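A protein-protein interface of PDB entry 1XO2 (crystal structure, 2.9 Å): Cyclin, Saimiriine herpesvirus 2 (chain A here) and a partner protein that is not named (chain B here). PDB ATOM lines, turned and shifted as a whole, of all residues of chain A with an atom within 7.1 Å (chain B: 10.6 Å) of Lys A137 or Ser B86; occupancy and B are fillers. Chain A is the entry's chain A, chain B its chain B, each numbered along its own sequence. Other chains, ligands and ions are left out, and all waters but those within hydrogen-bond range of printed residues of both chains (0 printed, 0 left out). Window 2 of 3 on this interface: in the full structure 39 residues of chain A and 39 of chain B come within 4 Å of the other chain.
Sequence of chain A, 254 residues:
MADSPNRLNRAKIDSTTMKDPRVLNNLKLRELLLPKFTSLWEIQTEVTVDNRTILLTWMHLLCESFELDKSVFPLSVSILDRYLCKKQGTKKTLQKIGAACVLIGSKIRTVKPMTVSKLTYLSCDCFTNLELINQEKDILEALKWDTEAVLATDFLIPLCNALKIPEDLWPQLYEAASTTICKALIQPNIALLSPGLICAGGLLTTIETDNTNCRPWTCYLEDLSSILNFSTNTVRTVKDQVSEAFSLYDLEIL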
ATOM      1  N   TYR A  83      11.156   7.305   8.469  1.00  0.00           N
ATOM      2  CA  TYR A  83       9.998   7.849   7.764  1.00  0.00           C
ATOM      3  C   TYR A  83      10.331   9.108   6.952  1.00  0.00           C
ATOM      4  O   TYR A  83       9.832   9.285   5.845  1.00  0.00           O
ATOM      5  CB  TYR A  83       8.890   8.212   8.747  1.00  0.00           C
ATOM      6  CG  TYR A  83       7.632   8.727   8.073  1.00  0.00           C
ATOM      7  CD1 TYR A  83       6.858   7.884   7.278  1.00  0.00           C
ATOM      8  CD2 TYR A  83       7.208  10.050   8.244  1.00  0.00           C
ATOM      9  CE1 TYR A  83       5.692   8.329   6.674  1.00  0.00           C
ATOM     10  CE2 TYR A  83       6.029  10.511   7.632  1.00  0.00           C
ATOM     11  CZ  TYR A  83       5.277   9.636   6.848  1.00  0.00           C
ATOM     12  OH  TYR A  83       4.105  10.043   6.242  1.00  0.00           O
ATOM     13  N   ALA A 100       3.012  10.763  16.295  1.00  0.00           N
ATOM     14  CA  ALA A 100       2.722   9.450  15.718  1.00  0.00           C
ATOM     15  C   ALA A 100       3.875   8.447  15.865  1.00  0.00           C
ATOM     16  O   ALA A 100       3.641   7.252  16.042  1.00  0.00           O
ATOM     17  CB  ALA A 100       2.345   9.608  14.241  1.00  0.00           C
ATOM     18  N   LEU A 103       3.682   7.351  19.356  1.00  0.00           N
ATOM     19  CA  LEU A 103       2.557   6.445  19.515  1.00  0.00           C
ATOM     20  C   LEU A 103       3.049   5.041  19.119  1.00  0.00           C
ATOM     21  O   LEU A 103       3.020   4.121  19.922  1.00  0.00           O
ATOM     22  CB  LEU A 103       1.405   6.870  18.607  1.00  0.00           C
ATOM     23  CG  LEU A 103       0.165   5.957  18.584  1.00  0.00           C
ATOM     24  CD1 LEU A 103      -0.590   6.047  19.909  1.00  0.00           C
ATOM     25  CD2 LEU A 103      -0.761   6.359  17.415  1.00  0.00           C
ATOM     26  N   ILE A 104       3.521   4.888  17.883  1.00  0.00           N
ATOM     27  CA  ILE A 104       4.008   3.599  17.399  1.00  0.00           C
ATOM     28  C   ILE A 104       5.109   3.038  18.304  1.00  0.00           C
ATOM     29  O   ILE A 104       5.009   1.922  18.830  1.00  0.00           O
ATOM     30  CB  ILE A 104       4.582   3.708  15.948  1.00  0.00           C
ATOM     31  CG1 ILE A 104       3.525   4.246  14.990  1.00  0.00           C
ATOM     32  CG2 ILE A 104       5.029   2.336  15.446  1.00  0.00           C
ATOM     33  CD1 ILE A 104       4.095   4.701  13.652  1.00  0.00           C
ATOM     34  N   LEU A 132      -4.252  11.937  13.928  1.00  0.00           N
ATOM     35  CA  LEU A 132      -3.110  11.257  14.514  1.00  0.00           C
ATOM     36  C   LEU A 132      -3.104   9.836  13.950  1.00  0.00           C
ATOM     37  O   LEU A 132      -2.065   9.325  13.515  1.00  0.00           O
ATOM     38  CB  LEU A 132      -3.265  11.193  16.031  1.00  0.00           C
ATOM     39  CG  LEU A 132      -2.030  11.506  16.875  1.00  0.00           C
ATOM     40  CD1 LEU A 132      -2.046  10.635  18.135  1.00  0.00           C
ATOM     41  CD2 LEU A 132      -0.765  11.255  16.073  1.00  0.00           C
ATOM     42  N   ILE A 133      -4.286   9.220  13.961  1.00  0.00           N
ATOM     43  CA  ILE A 133      -4.496   7.863  13.469  1.00  0.00           C
ATOM     44  C   ILE A 133      -4.141   7.669  11.996  1.00  0.00           C
ATOM     45  O   ILE A 133      -3.489   6.682  11.632  1.00  0.00           O
ATOM     46  CB  ILE A 133      -5.953   7.428  13.697  1.00  0.00           C
ATOM     47  CG1 ILE A 133      -6.219   7.344  15.207  1.00  0.00           C
ATOM     48  CG2 ILE A 133      -6.223   6.100  12.983  1.00  0.00           C
ATOM     49  CD1 ILE A 133      -7.596   6.844  15.576  1.00  0.00           C
ATOM     50  N   ASN A 134      -4.569   8.593  11.145  1.00  0.00           N
ATOM     51  CA  ASN A 134      -4.236   8.461   9.739  1.00  0.00           C
ATOM     52  C   ASN A 134      -2.748   8.706   9.573  1.00  0.00           C
ATOM     53  O   ASN A 134      -2.168   8.340   8.560  1.00  0.00           O
ATOM     54  CB  ASN A 134      -5.039   9.447   8.876  1.00  0.00           C
ATOM     55  CG  ASN A 134      -6.513   9.067   8.762  1.00  0.00           C
ATOM     56  OD1 ASN A 134      -6.855   7.925   8.436  1.00  0.00           O
ATOM     57  ND2 ASN A 134      -7.394  10.030   9.023  1.00  0.00           N
ATOM     58  N   GLN A 135      -2.125   9.319  10.574  1.00  0.00           N
ATOM     59  CA  GLN A 135      -0.697   9.607  10.515  1.00  0.00           C
ATOM     60  C   GLN A 135       0.082   8.352  10.887  1.00  0.00           C
ATOM     61  O   GLN A 135       1.082   8.015  10.244  1.00  0.00           O
ATOM     62  CB  GLN A 135      -0.345  10.754  11.463  1.00  0.00           C
ATOM     63  CG  GLN A 135       1.044  11.359  11.250  1.00  0.00           C
ATOM     64  CD  GLN A 135       1.264  11.894   9.836  1.00  0.00           C
ATOM     65  OE1 GLN A 135       0.390  12.533   9.252  1.00  0.00           O
ATOM     66  NE2 GLN A 135       2.447  11.646   9.292  1.00  0.00           N
ATOM     67  N   GLU A 136      -0.377   7.662  11.926  1.00  0.00           N
ATOM     68  CA  GLU A 136       0.270   6.425  12.352  1.00  0.00           C
ATOM     69  C   GLU A 136       0.274   5.479  11.143  1.00  0.00           C
ATOM     70  O   GLU A 136       1.286   4.846  10.824  1.00  0.00           O
ATOM     71  CB  GLU A 136      -0.513   5.813  13.510  1.00  0.00           C
ATOM     72  CG  GLU A 136      -0.065   4.416  13.895  1.00  0.00           C
ATOM     73  CD  GLU A 136      -0.981   3.772  14.932  1.00  0.00           C
ATOM     74  OE1 GLU A 136      -2.200   3.645  14.664  1.00  0.00           O
ATOM     75  OE2 GLU A 136      -0.478   3.393  16.015  1.00  0.00           O
ATOM     76  N   LYS A 137      -0.876   5.407  10.476  1.00  0.00           N
ATOM     77  CA  LYS A 137      -1.063   4.589   9.286  1.00  0.00           C
ATOM     78  C   LYS A 137      -0.068   4.966   8.184  1.00  0.00           C
ATOM     79  O   LYS A 137       0.735   4.141   7.751  1.00  0.00           O
ATOM     80  CB  LYS A 137      -2.483   4.781   8.766  1.00  0.00           C
ATOM     81  CG  LYS A 137      -2.785   4.030   7.486  1.00  0.00           C
ATOM     82  CD  LYS A 137      -4.108   4.478   6.865  1.00  0.00           C
ATOM     83  CE  LYS A 137      -4.030   5.917   6.340  1.00  0.00           C
ATOM     84  NZ  LYS A 137      -5.281   6.339   5.638  1.00  0.00           N
ATOM     85  N   ASP A 138      -0.129   6.214   7.733  1.00  0.00           N
ATOM     86  CA  ASP A 138       0.755   6.689   6.674  1.00  0.00           C
ATOM     87  C   ASP A 138       2.221   6.417   6.954  1.00  0.00           C
ATOM     88  O   ASP A 138       3.020   6.323   6.024  1.00  0.00           O
ATOM     89  CB  ASP A 138       0.570   8.192   6.429  1.00  0.00           C
ATOM     90  CG  ASP A 138      -0.603   8.510   5.502  1.00  0.00           C
ATOM     91  OD1 ASP A 138      -1.771   8.242   5.864  1.00  0.00           O
ATOM     92  OD2 ASP A 138      -0.344   9.038   4.402  1.00  0.00           O
ATOM     93  N   ILE A 139       2.583   6.308   8.228  1.00  0.00           N
ATOM     94  CA  ILE A 139       3.974   6.037   8.597  1.00  0.00           C
ATOM     95  C   ILE A 139       4.301   4.561   8.410  1.00  0.00           C
ATOM     96  O   ILE A 139       5.364   4.208   7.891  1.00  0.00           O
ATOM     97  CB  ILE A 139       4.251   6.450  10.067  1.00  0.00           C
ATOM     98  CG1 ILE A 139       4.175   7.977  10.168  1.00  0.00           C
ATOM     99  CG2 ILE A 139       5.618   5.912  10.540  1.00  0.00           C
ATOM    100  CD1 ILE A 139       4.140   8.509  11.580  1.00  0.00           C
ATOM    101  N   LEU A 140       3.364   3.711   8.820  1.00  0.00           N
ATOM    102  CA  LEU A 140       3.529   2.268   8.714  1.00  0.00           C
ATOM    103  C   LEU A 140       3.635   1.799   7.267  1.00  0.00           C
ATOM    104  O   LEU A 140       4.604   1.122   6.884  1.00  0.00           O
ATOM    105  CB  LEU A 140       2.371   1.557   9.419  1.00  0.00           C
ATOM    106  CG  LEU A 140       2.395   1.627  10.951  1.00  0.00           C
ATOM    107  CD1 LEU A 140       1.172   0.945  11.555  1.00  0.00           C
ATOM    108  CD2 LEU A 140       3.674   0.973  11.441  1.00  0.00           C
ATOM    109  N   GLU A 141       2.650   2.168   6.457  1.00  0.00           N
ATOM    110  CA  GLU A 141       2.656   1.772   5.059  1.00  0.00           C
ATOM    111  C   GLU A 141       3.963   2.206   4.434  1.00  0.00           C
ATOM    112  O   GLU A 141       4.547   1.479   3.639  1.00  0.00           O
ATOM    113  CB  GLU A 141       1.474   2.401   4.323  1.00  0.00           C
ATOM    114  CG  GLU A 141       1.427   3.908   4.388  1.00  0.00           C
ATOM    115  CD  GLU A 141       0.021   4.446   4.182  1.00  0.00           C
ATOM    116  OE1 GLU A 141      -0.129   5.673   3.993  1.00  0.00           O
ATOM    117  OE2 GLU A 141      -0.936   3.641   4.220  1.00  0.00           O
ATOM    118  N   ALA A 142       4.425   3.387   4.829  1.00  0.00           N
ATOM    119  CA  ALA A 142       5.667   3.966   4.327  1.00  0.00           C
ATOM    120  C   ALA A 142       6.880   3.101   4.633  1.00  0.00           C
ATOM    121  O   ALA A 142       7.782   2.955   3.808  1.00  0.00           O
ATOM    122  CB  ALA A 142       5.859   5.347   4.921  1.00  0.00           C
ATOM    123  N   LEU A 143       6.889   2.528   5.832  1.00  0.00           N
ATOM    124  CA  LEU A 143       7.994   1.680   6.258  1.00  0.00           C
ATOM    125  C   LEU A 143       7.700   0.209   6.033  1.00  0.00           C
ATOM    126  O   LEU A 143       8.438  -0.657   6.513  1.00  0.00           O
ATOM    127  CB  LEU A 143       8.310   1.917   7.735  1.00  0.00           C
ATOM    128  CG  LEU A 143       8.700   3.345   8.119  1.00  0.00           C
ATOM    129  CD1 LEU A 143       9.319   3.320   9.509  1.00  0.00           C
ATOM    130  CD2 LEU A 143       9.679   3.921   7.099  1.00  0.00           C
ATOM    131  N   TRP A 145       5.561  -1.521   7.307  1.00  0.00           N
ATOM    132  CA  TRP A 145       5.349  -2.063   8.638  1.00  0.00           C
ATOM    133  C   TRP A 145       6.625  -2.530   9.329  1.00  0.00           C
ATOM    134  O   TRP A 145       6.576  -3.076  10.436  1.00  0.00           O
ATOM    135  CB  TRP A 145       4.300  -3.191   8.597  1.00  0.00           C
ATOM    136  CG  TRP A 145       2.882  -2.663   8.414  1.00  0.00           C
ATOM    137  CD1 TRP A 145       2.350  -2.121   7.279  1.00  0.00           C
ATOM    138  CD2 TRP A 145       1.868  -2.547   9.423  1.00  0.00           C
ATOM    139  NE1 TRP A 145       1.077  -1.675   7.522  1.00  0.00           N
ATOM    140  CE2 TRP A 145       0.757  -1.923   8.829  1.00  0.00           C
ATOM    141  CE3 TRP A 145       1.795  -2.906  10.767  1.00  0.00           C
ATOM    142  CZ2 TRP A 145      -0.419  -1.650   9.535  1.00  0.00           C
ATOM    143  CZ3 TRP A 145       0.627  -2.636  11.471  1.00  0.00           C
ATOM    144  CH2 TRP A 145      -0.467  -2.014  10.850  1.00  0.00           C
ATOM    145  N   VAL B  45      -7.334  -8.673  11.443  1.00  0.00           N
ATOM    146  CA  VAL B  45      -7.675  -8.078  12.734  1.00  0.00           C
ATOM    147  C   VAL B  45      -8.690  -6.947  12.569  1.00  0.00           C
ATOM    148  O   VAL B  45      -8.534  -6.088  11.700  1.00  0.00           O
ATOM    149  CB  VAL B  45      -6.419  -7.503  13.422  1.00  0.00           C
ATOM    150  CG1 VAL B  45      -6.766  -7.039  14.826  1.00  0.00           C
ATOM    151  CG2 VAL B  45      -5.319  -8.546  13.461  1.00  0.00           C
ATOM    152  N   VAL B  47      -9.824  -3.694  13.254  1.00  0.00           N
ATOM    153  CA  VAL B  47      -9.326  -2.420  13.766  1.00  0.00           C
ATOM    154  C   VAL B  47     -10.462  -1.417  13.949  1.00  0.00           C
ATOM    155  O   VAL B  47     -10.541  -0.411  13.244  1.00  0.00           O
ATOM    156  CB  VAL B  47      -8.277  -1.821  12.804  1.00  0.00           C
ATOM    157  CG1 VAL B  47      -7.672  -0.562  13.400  1.00  0.00           C
ATOM    158  CG2 VAL B  47      -7.200  -2.848  12.519  1.00  0.00           C
ATOM    159  N   GLN B  48     -11.337  -1.697  14.906  1.00  0.00           N
ATOM    160  CA  GLN B  48     -12.475  -0.830  15.180  1.00  0.00           C
ATOM    161  C   GLN B  48     -12.002   0.597  15.414  1.00  0.00           C
ATOM    162  O   GLN B  48     -10.996   0.822  16.088  1.00  0.00           O
ATOM    163  CB  GLN B  48     -13.242  -1.352  16.397  1.00  0.00           C
ATOM    164  CG  GLN B  48     -13.417  -2.868  16.375  1.00  0.00           C
ATOM    165  CD  GLN B  48     -14.338  -3.376  17.460  1.00  0.00           C
ATOM    166  OE1 GLN B  48     -14.293  -2.909  18.599  1.00  0.00           O
ATOM    167  NE2 GLN B  48     -15.173  -4.350  17.116  1.00  0.00           N
ATOM    168  N   THR B  49     -12.730   1.555  14.847  1.00  0.00           N
ATOM    169  CA  THR B  49     -12.393   2.969  14.969  1.00  0.00           C
ATOM    170  C   THR B  49     -12.569   3.519  16.380  1.00  0.00           C
ATOM    171  O   THR B  49     -13.159   4.587  16.569  1.00  0.00           O
ATOM    172  CB  THR B  49     -13.239   3.824  14.008  1.00  0.00           C
ATOM    173  OG1 THR B  49     -14.630   3.580  14.247  1.00  0.00           O
ATOM    174  CG2 THR B  49     -12.907   3.484  12.566  1.00  0.00           C
ATOM    175  N   GLU B  52      -7.591   4.290  19.370  1.00  0.00           N
ATOM    176  CA  GLU B  52      -6.211   3.945  19.667  1.00  0.00           C
ATOM    177  C   GLU B  52      -5.344   3.699  18.446  1.00  0.00           C
ATOM    178  O   GLU B  52      -4.136   3.528  18.569  1.00  0.00           O
ATOM    179  CB  GLU B  52      -6.163   2.733  20.592  1.00  0.00           C
ATOM    180  CG  GLU B  52      -6.747   2.999  21.970  1.00  0.00           C
ATOM    181  CD  GLU B  52      -6.263   4.310  22.576  1.00  0.00           C
ATOM    182  OE1 GLU B  52      -5.098   4.686  22.333  1.00  0.00           O
ATOM    183  OE2 GLU B  52      -7.047   4.957  23.303  1.00  0.00           O
ATOM    184  N   GLY B  53      -5.953   3.695  17.267  1.00  0.00           N
ATOM    185  CA  GLY B  53      -5.195   3.462  16.052  1.00  0.00           C
ATOM    186  C   GLY B  53      -4.944   1.983  15.846  1.00  0.00           C
ATOM    187  O   GLY B  53      -5.675   1.145  16.372  1.00  0.00           O
ATOM    188  N   MET B  54      -3.901   1.655  15.096  1.00  0.00           N
ATOM    189  CA  MET B  54      -3.569   0.262  14.829  1.00  0.00           C
ATOM    190  C   MET B  54      -3.322  -0.546  16.100  1.00  0.00           C
ATOM    191  O   MET B  54      -2.635  -0.100  17.014  1.00  0.00           O
ATOM    192  CB  MET B  54      -2.346   0.183  13.922  1.00  0.00           C
ATOM    193  CG  MET B  54      -2.584   0.775  12.554  1.00  0.00           C
ATOM    194  SD  MET B  54      -3.900  -0.077  11.640  1.00  0.00           S
ATOM    195  CE  MET B  54      -3.407   0.343   9.925  1.00  0.00           C
ATOM    196  N   PRO B  55      -3.891  -1.760  16.165  1.00  0.00           N
ATOM    197  CA  PRO B  55      -3.738  -2.637  17.328  1.00  0.00           C
ATOM    198  C   PRO B  55      -2.282  -2.993  17.615  1.00  0.00           C
ATOM    199  O   PRO B  55      -1.568  -3.501  16.751  1.00  0.00           O
ATOM    200  CB  PRO B  55      -4.570  -3.856  16.948  1.00  0.00           C
ATOM    201  CG  PRO B  55      -5.623  -3.283  16.027  1.00  0.00           C
ATOM    202  CD  PRO B  55      -4.796  -2.367  15.170  1.00  0.00           C
ATOM    203  N   ILE B  59       1.018  -4.792  15.482  1.00  0.00           N
ATOM    204  CA  ILE B  59       2.251  -4.063  15.221  1.00  0.00           C
ATOM    205  C   ILE B  59       3.485  -4.793  15.724  1.00  0.00           C
ATOM    206  O   ILE B  59       4.379  -5.086  14.922  1.00  0.00           O
ATOM    207  CB  ILE B  59       2.189  -2.620  15.771  1.00  0.00           C
ATOM    208  CG1 ILE B  59       0.975  -1.915  15.171  1.00  0.00           C
ATOM    209  CG2 ILE B  59       3.400  -1.806  15.285  1.00  0.00           C
ATOM    210  CD1 ILE B  59       1.009  -0.407  15.331  1.00  0.00           C
ATOM    211  N   VAL B  82       0.642  -7.420   4.352  1.00  0.00           N
ATOM    212  CA  VAL B  82      -0.258  -6.744   5.271  1.00  0.00           C
ATOM    213  C   VAL B  82      -1.222  -5.911   4.432  1.00  0.00           C
ATOM    214  O   VAL B  82      -0.811  -4.943   3.805  1.00  0.00           O
ATOM    215  CB  VAL B  82       0.531  -5.808   6.201  1.00  0.00           C
ATOM    216  CG1 VAL B  82      -0.397  -5.147   7.216  1.00  0.00           C
ATOM    217  CG2 VAL B  82       1.621  -6.588   6.898  1.00  0.00           C
ATOM    218  N   CYS B  83      -2.493  -6.308   4.406  1.00  0.00           N
ATOM    219  CA  CYS B  83      -3.531  -5.597   3.650  1.00  0.00           C
ATOM    220  C   CYS B  83      -4.388  -4.768   4.591  1.00  0.00           C
ATOM    221  O   CYS B  83      -4.723  -5.209   5.690  1.00  0.00           O
ATOM    222  CB  CYS B  83      -4.443  -6.576   2.903  1.00  0.00           C
ATOM    223  SG  CYS B  83      -3.832  -7.158   1.314  1.00  0.00           S
ATOM    224  N   THR B  84      -4.760  -3.573   4.148  1.00  0.00           N
ATOM    225  CA  THR B  84      -5.579  -2.688   4.964  1.00  0.00           C
ATOM    226  C   THR B  84      -6.569  -1.875   4.146  1.00  0.00           C
ATOM    227  O   THR B  84      -6.178  -1.143   3.238  1.00  0.00           O
ATOM    228  CB  THR B  84      -4.706  -1.702   5.754  1.00  0.00           C
ATOM    229  OG1 THR B  84      -3.783  -1.065   4.862  1.00  0.00           O
ATOM    230  CG2 THR B  84      -3.943  -2.421   6.847  1.00  0.00           C
ATOM    231  N   VAL B  85      -7.852  -2.006   4.470  1.00  0.00           N
ATOM    232  CA  VAL B  85      -8.891  -1.249   3.780  1.00  0.00           C
ATOM    233  C   VAL B  85      -9.309  -0.115   4.721  1.00  0.00           C
ATOM    234  O   VAL B  85      -9.773  -0.365   5.835  1.00  0.00           O
ATOM    235  CB  VAL B  85     -10.124  -2.121   3.460  1.00  0.00           C
ATOM    236  CG1 VAL B  85     -11.097  -1.336   2.596  1.00  0.00           C
ATOM    237  CG2 VAL B  85      -9.693  -3.395   2.752  1.00  0.00           C
ATOM    238  N   SER B  86      -9.133   1.124   4.266  1.00  0.00           N
ATOM    239  CA  SER B  86      -9.461   2.314   5.059  1.00  0.00           C
ATOM    240  C   SER B  86     -10.960   2.599   5.182  1.00  0.00           C
ATOM    241  O   SER B  86     -11.369   3.515   5.900  1.00  0.00           O
ATOM    242  CB  SER B  86      -8.760   3.543   4.464  1.00  0.00           C
ATOM    243  OG  SER B  86      -7.353   3.372   4.432  1.00  0.00           O
ATOM    244  N   ARG B  87     -11.770   1.811   4.482  1.00  0.00           N
ATOM    245  CA  ARG B  87     -13.220   1.968   4.499  1.00  0.00           C
ATOM    246  C   ARG B  87     -13.753   2.276   5.892  1.00  0.00           C
ATOM    247  O   ARG B  87     -13.890   3.440   6.270  1.00  0.00           O
ATOM    248  CB  ARG B  87     -13.888   0.698   3.959  1.00  0.00           C
ATOM    249  CG  ARG B  87     -13.576  -0.572   4.746  1.00  0.00           C
ATOM    250  CD  ARG B  87     -14.173  -1.796   4.061  1.00  0.00           C
ATOM    251  NE  ARG B  87     -13.833  -3.049   4.735  1.00  0.00           N
ATOM    252  CZ  ARG B  87     -14.338  -3.443   5.901  1.00  0.00           C
ATOM    253  NH1 ARG B  87     -15.218  -2.681   6.543  1.00  0.00           N
ATOM    254  NH2 ARG B  87     -13.966  -4.605   6.424  1.00  0.00           N
ATOM    255  N   GLU B  91     -15.558   0.774  10.704  1.00  0.00           N
ATOM    256  CA  GLU B  91     -14.195   0.473  11.121  1.00  0.00           C
ATOM    257  C   GLU B  91     -13.316   0.148   9.918  1.00  0.00           C
ATOM    258  O   GLU B  91     -13.778   0.142   8.775  1.00  0.00           O
ATOM    259  CB  GLU B  91     -14.183  -0.715  12.090  1.00  0.00           C
ATOM    260  CG  GLU B  91     -14.677  -2.023  11.485  1.00  0.00           C
ATOM    261  CD  GLU B  91     -14.398  -3.229  12.368  1.00  0.00           C
ATOM    262  OE1 GLU B  91     -14.908  -3.268  13.508  1.00  0.00           O
ATOM    263  OE2 GLU B  91     -13.667  -4.140  11.920  1.00  0.00           O
ATOM    264  N   THR B  92     -12.043  -0.117  10.187  1.00  0.00           N
ATOM    265  CA  THR B  92     -11.092  -0.471   9.141  1.00  0.00           C
ATOM    266  C   THR B  92     -10.755  -1.951   9.314  1.00  0.00           C
ATOM    267  O   THR B  92     -10.826  -2.488  10.420  1.00  0.00           O
ATOM    268  CB  THR B  92      -9.792   0.337   9.263  1.00  0.00           C
ATOM    269  OG1 THR B  92      -8.920  -0.308  10.198  1.00  0.00           O
ATOM    270  CG2 THR B  92     -10.093   1.747   9.750  1.00  0.00           C
ATOM    271  N   LYS B  93     -10.398  -2.612   8.220  1.00  0.00           N
ATOM    272  CA  LYS B  93     -10.054  -4.025   8.279  1.00  0.00           C
ATOM    273  C   LYS B  93      -8.579  -4.267   7.969  1.00  0.00           C
ATOM    274  O   LYS B  93      -8.101  -4.015   6.859  1.00  0.00           O
ATOM    275  CB  LYS B  93     -10.936  -4.833   7.314  1.00  0.00           C
ATOM    276  CG  LYS B  93     -10.865  -4.410   5.846  1.00  0.00           C
ATOM    277  CD  LYS B  93     -11.488  -5.461   4.920  1.00  0.00           C
ATOM    278  CE  LYS B  93     -10.698  -6.774   4.942  1.00  0.00           C
ATOM    279  NZ  LYS B  93     -11.286  -7.835   4.071  1.00  0.00           N
ATOM    280  N   LEU B  94      -7.864  -4.760   8.974  1.00  0.00           N
ATOM    281  CA  LEU B  94      -6.440  -5.048   8.844  1.00  0.00           C
ATOM    282  C   LEU B  94      -6.253  -6.543   8.584  1.00  0.00           C
ATOM    283  O   LEU B  94      -6.494  -7.369   9.466  1.00  0.00           O
ATOM    284  CB  LEU B  94      -5.715  -4.660  10.137  1.00  0.00           C
ATOM    285  CG  LEU B  94      -4.386  -3.911  10.048  1.00  0.00           C
ATOM    286  CD1 LEU B  94      -3.838  -3.710  11.445  1.00  0.00           C
ATOM    287  CD2 LEU B  94      -3.400  -4.688   9.210  1.00  0.00           C
ATOM    288  N   THR B  95      -5.834  -6.893   7.374  1.00  0.00           N
ATOM    289  CA  THR B  95      -5.613  -8.293   7.049  1.00  0.00           C
ATOM    290  C   THR B  95      -4.135  -8.610   6.858  1.00  0.00           C
ATOM    291  O   THR B  95      -3.501  -8.169   5.907  1.00  0.00           O
ATOM    292  CB  THR B  95      -6.409  -8.706   5.798  1.00  0.00           C
ATOM    293  OG1 THR B  95      -7.775  -8.932   6.165  1.00  0.00           O
ATOM    294  CG2 THR B  95      -5.839  -9.974   5.183  1.00  0.00           C
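Among the printed residues, pairs that only touch across the chains: Ile A133 with Gly B53, Glu A136 with Gly B53, Lys A137 with Ser B86, Leu A140 with Met B54, Trp A145 with Met B54, Trp A145 with Ile B59, Trp A145 with Val B82 and Trp A145 with Leu B94.
Printed residues of chain A that touch a printed residue of chain B: Ile A133, Glu A136, Lys A137, Leu A140 and Trp A145. Hydrophobic or aromatic side chains of chain A that line the printed part of chain B: Ile A133, Leu A140 and Trp A145. Along chain A the printed residues that touch a printed residue of chain B span positions 133 to 145. Printed residues of chain B that touch a printed residue of chain A: Gly B53, Met B54, Ile B59, Val B82, Ser B86 and Leu B94. Hydrophobic or aromatic side chains of chain B that line the printed part of chain A: Met B54, Ile B59, Val B82 and Leu B94.
N of Met B54 lies within hydrogen-bond range of OE1 of Glu A136 (2.7 Å).
O of Leu A140 lies within hydrogen-bond range of N of Trp A145. The backbone NH (N) of Val B45 lies within hydrogen-bond range of the backbone carbonyl oxygen (O) of Leu B94, 2.5 Å away. OD1 of Asp A138 is in salt-bridge range of NZ of Lys A137 (3.999 Å).
No residue of chain B comes within 4 Å of Asn A134. Printed residues of chain B within 4 Å of Lys A137: Ser B86. No residue of chain B comes within 4 Å of Asp A138. No residue of chain B comes within 4 Å of Ile A139. Of the printed residues of chain B, Trp A145 touches Met B54 (3.6 Å), Ile B59 (3.8 Å), Val B82 (3.8 Å) and Leu B94 (3.8 Å). Printed residues of chain A within 4 Å of Met B54: Glu A136 (2.7 Å), Leu A140 (3.9 Å) and Trp A145 (3.6 Å). Of the printed residues of chain A, Ile B59 touches Trp A145. Ser B86 touches one residue of chain A. Thr B92 touches none of the printed residues of chain A. Of the printed residues of chain A, Leu B94 touches Trp A145 (3.8 Å). The nearest residue of chain B that does not touch Lys A137 is Met B54 (4.5 Å). The nearest residue of chain A that does not touch Ser B86 is Asn A134 (6.1 Å). The nearest printed residue of chain A that does not touch Val B82 is Leu A140 (7.6 Å).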
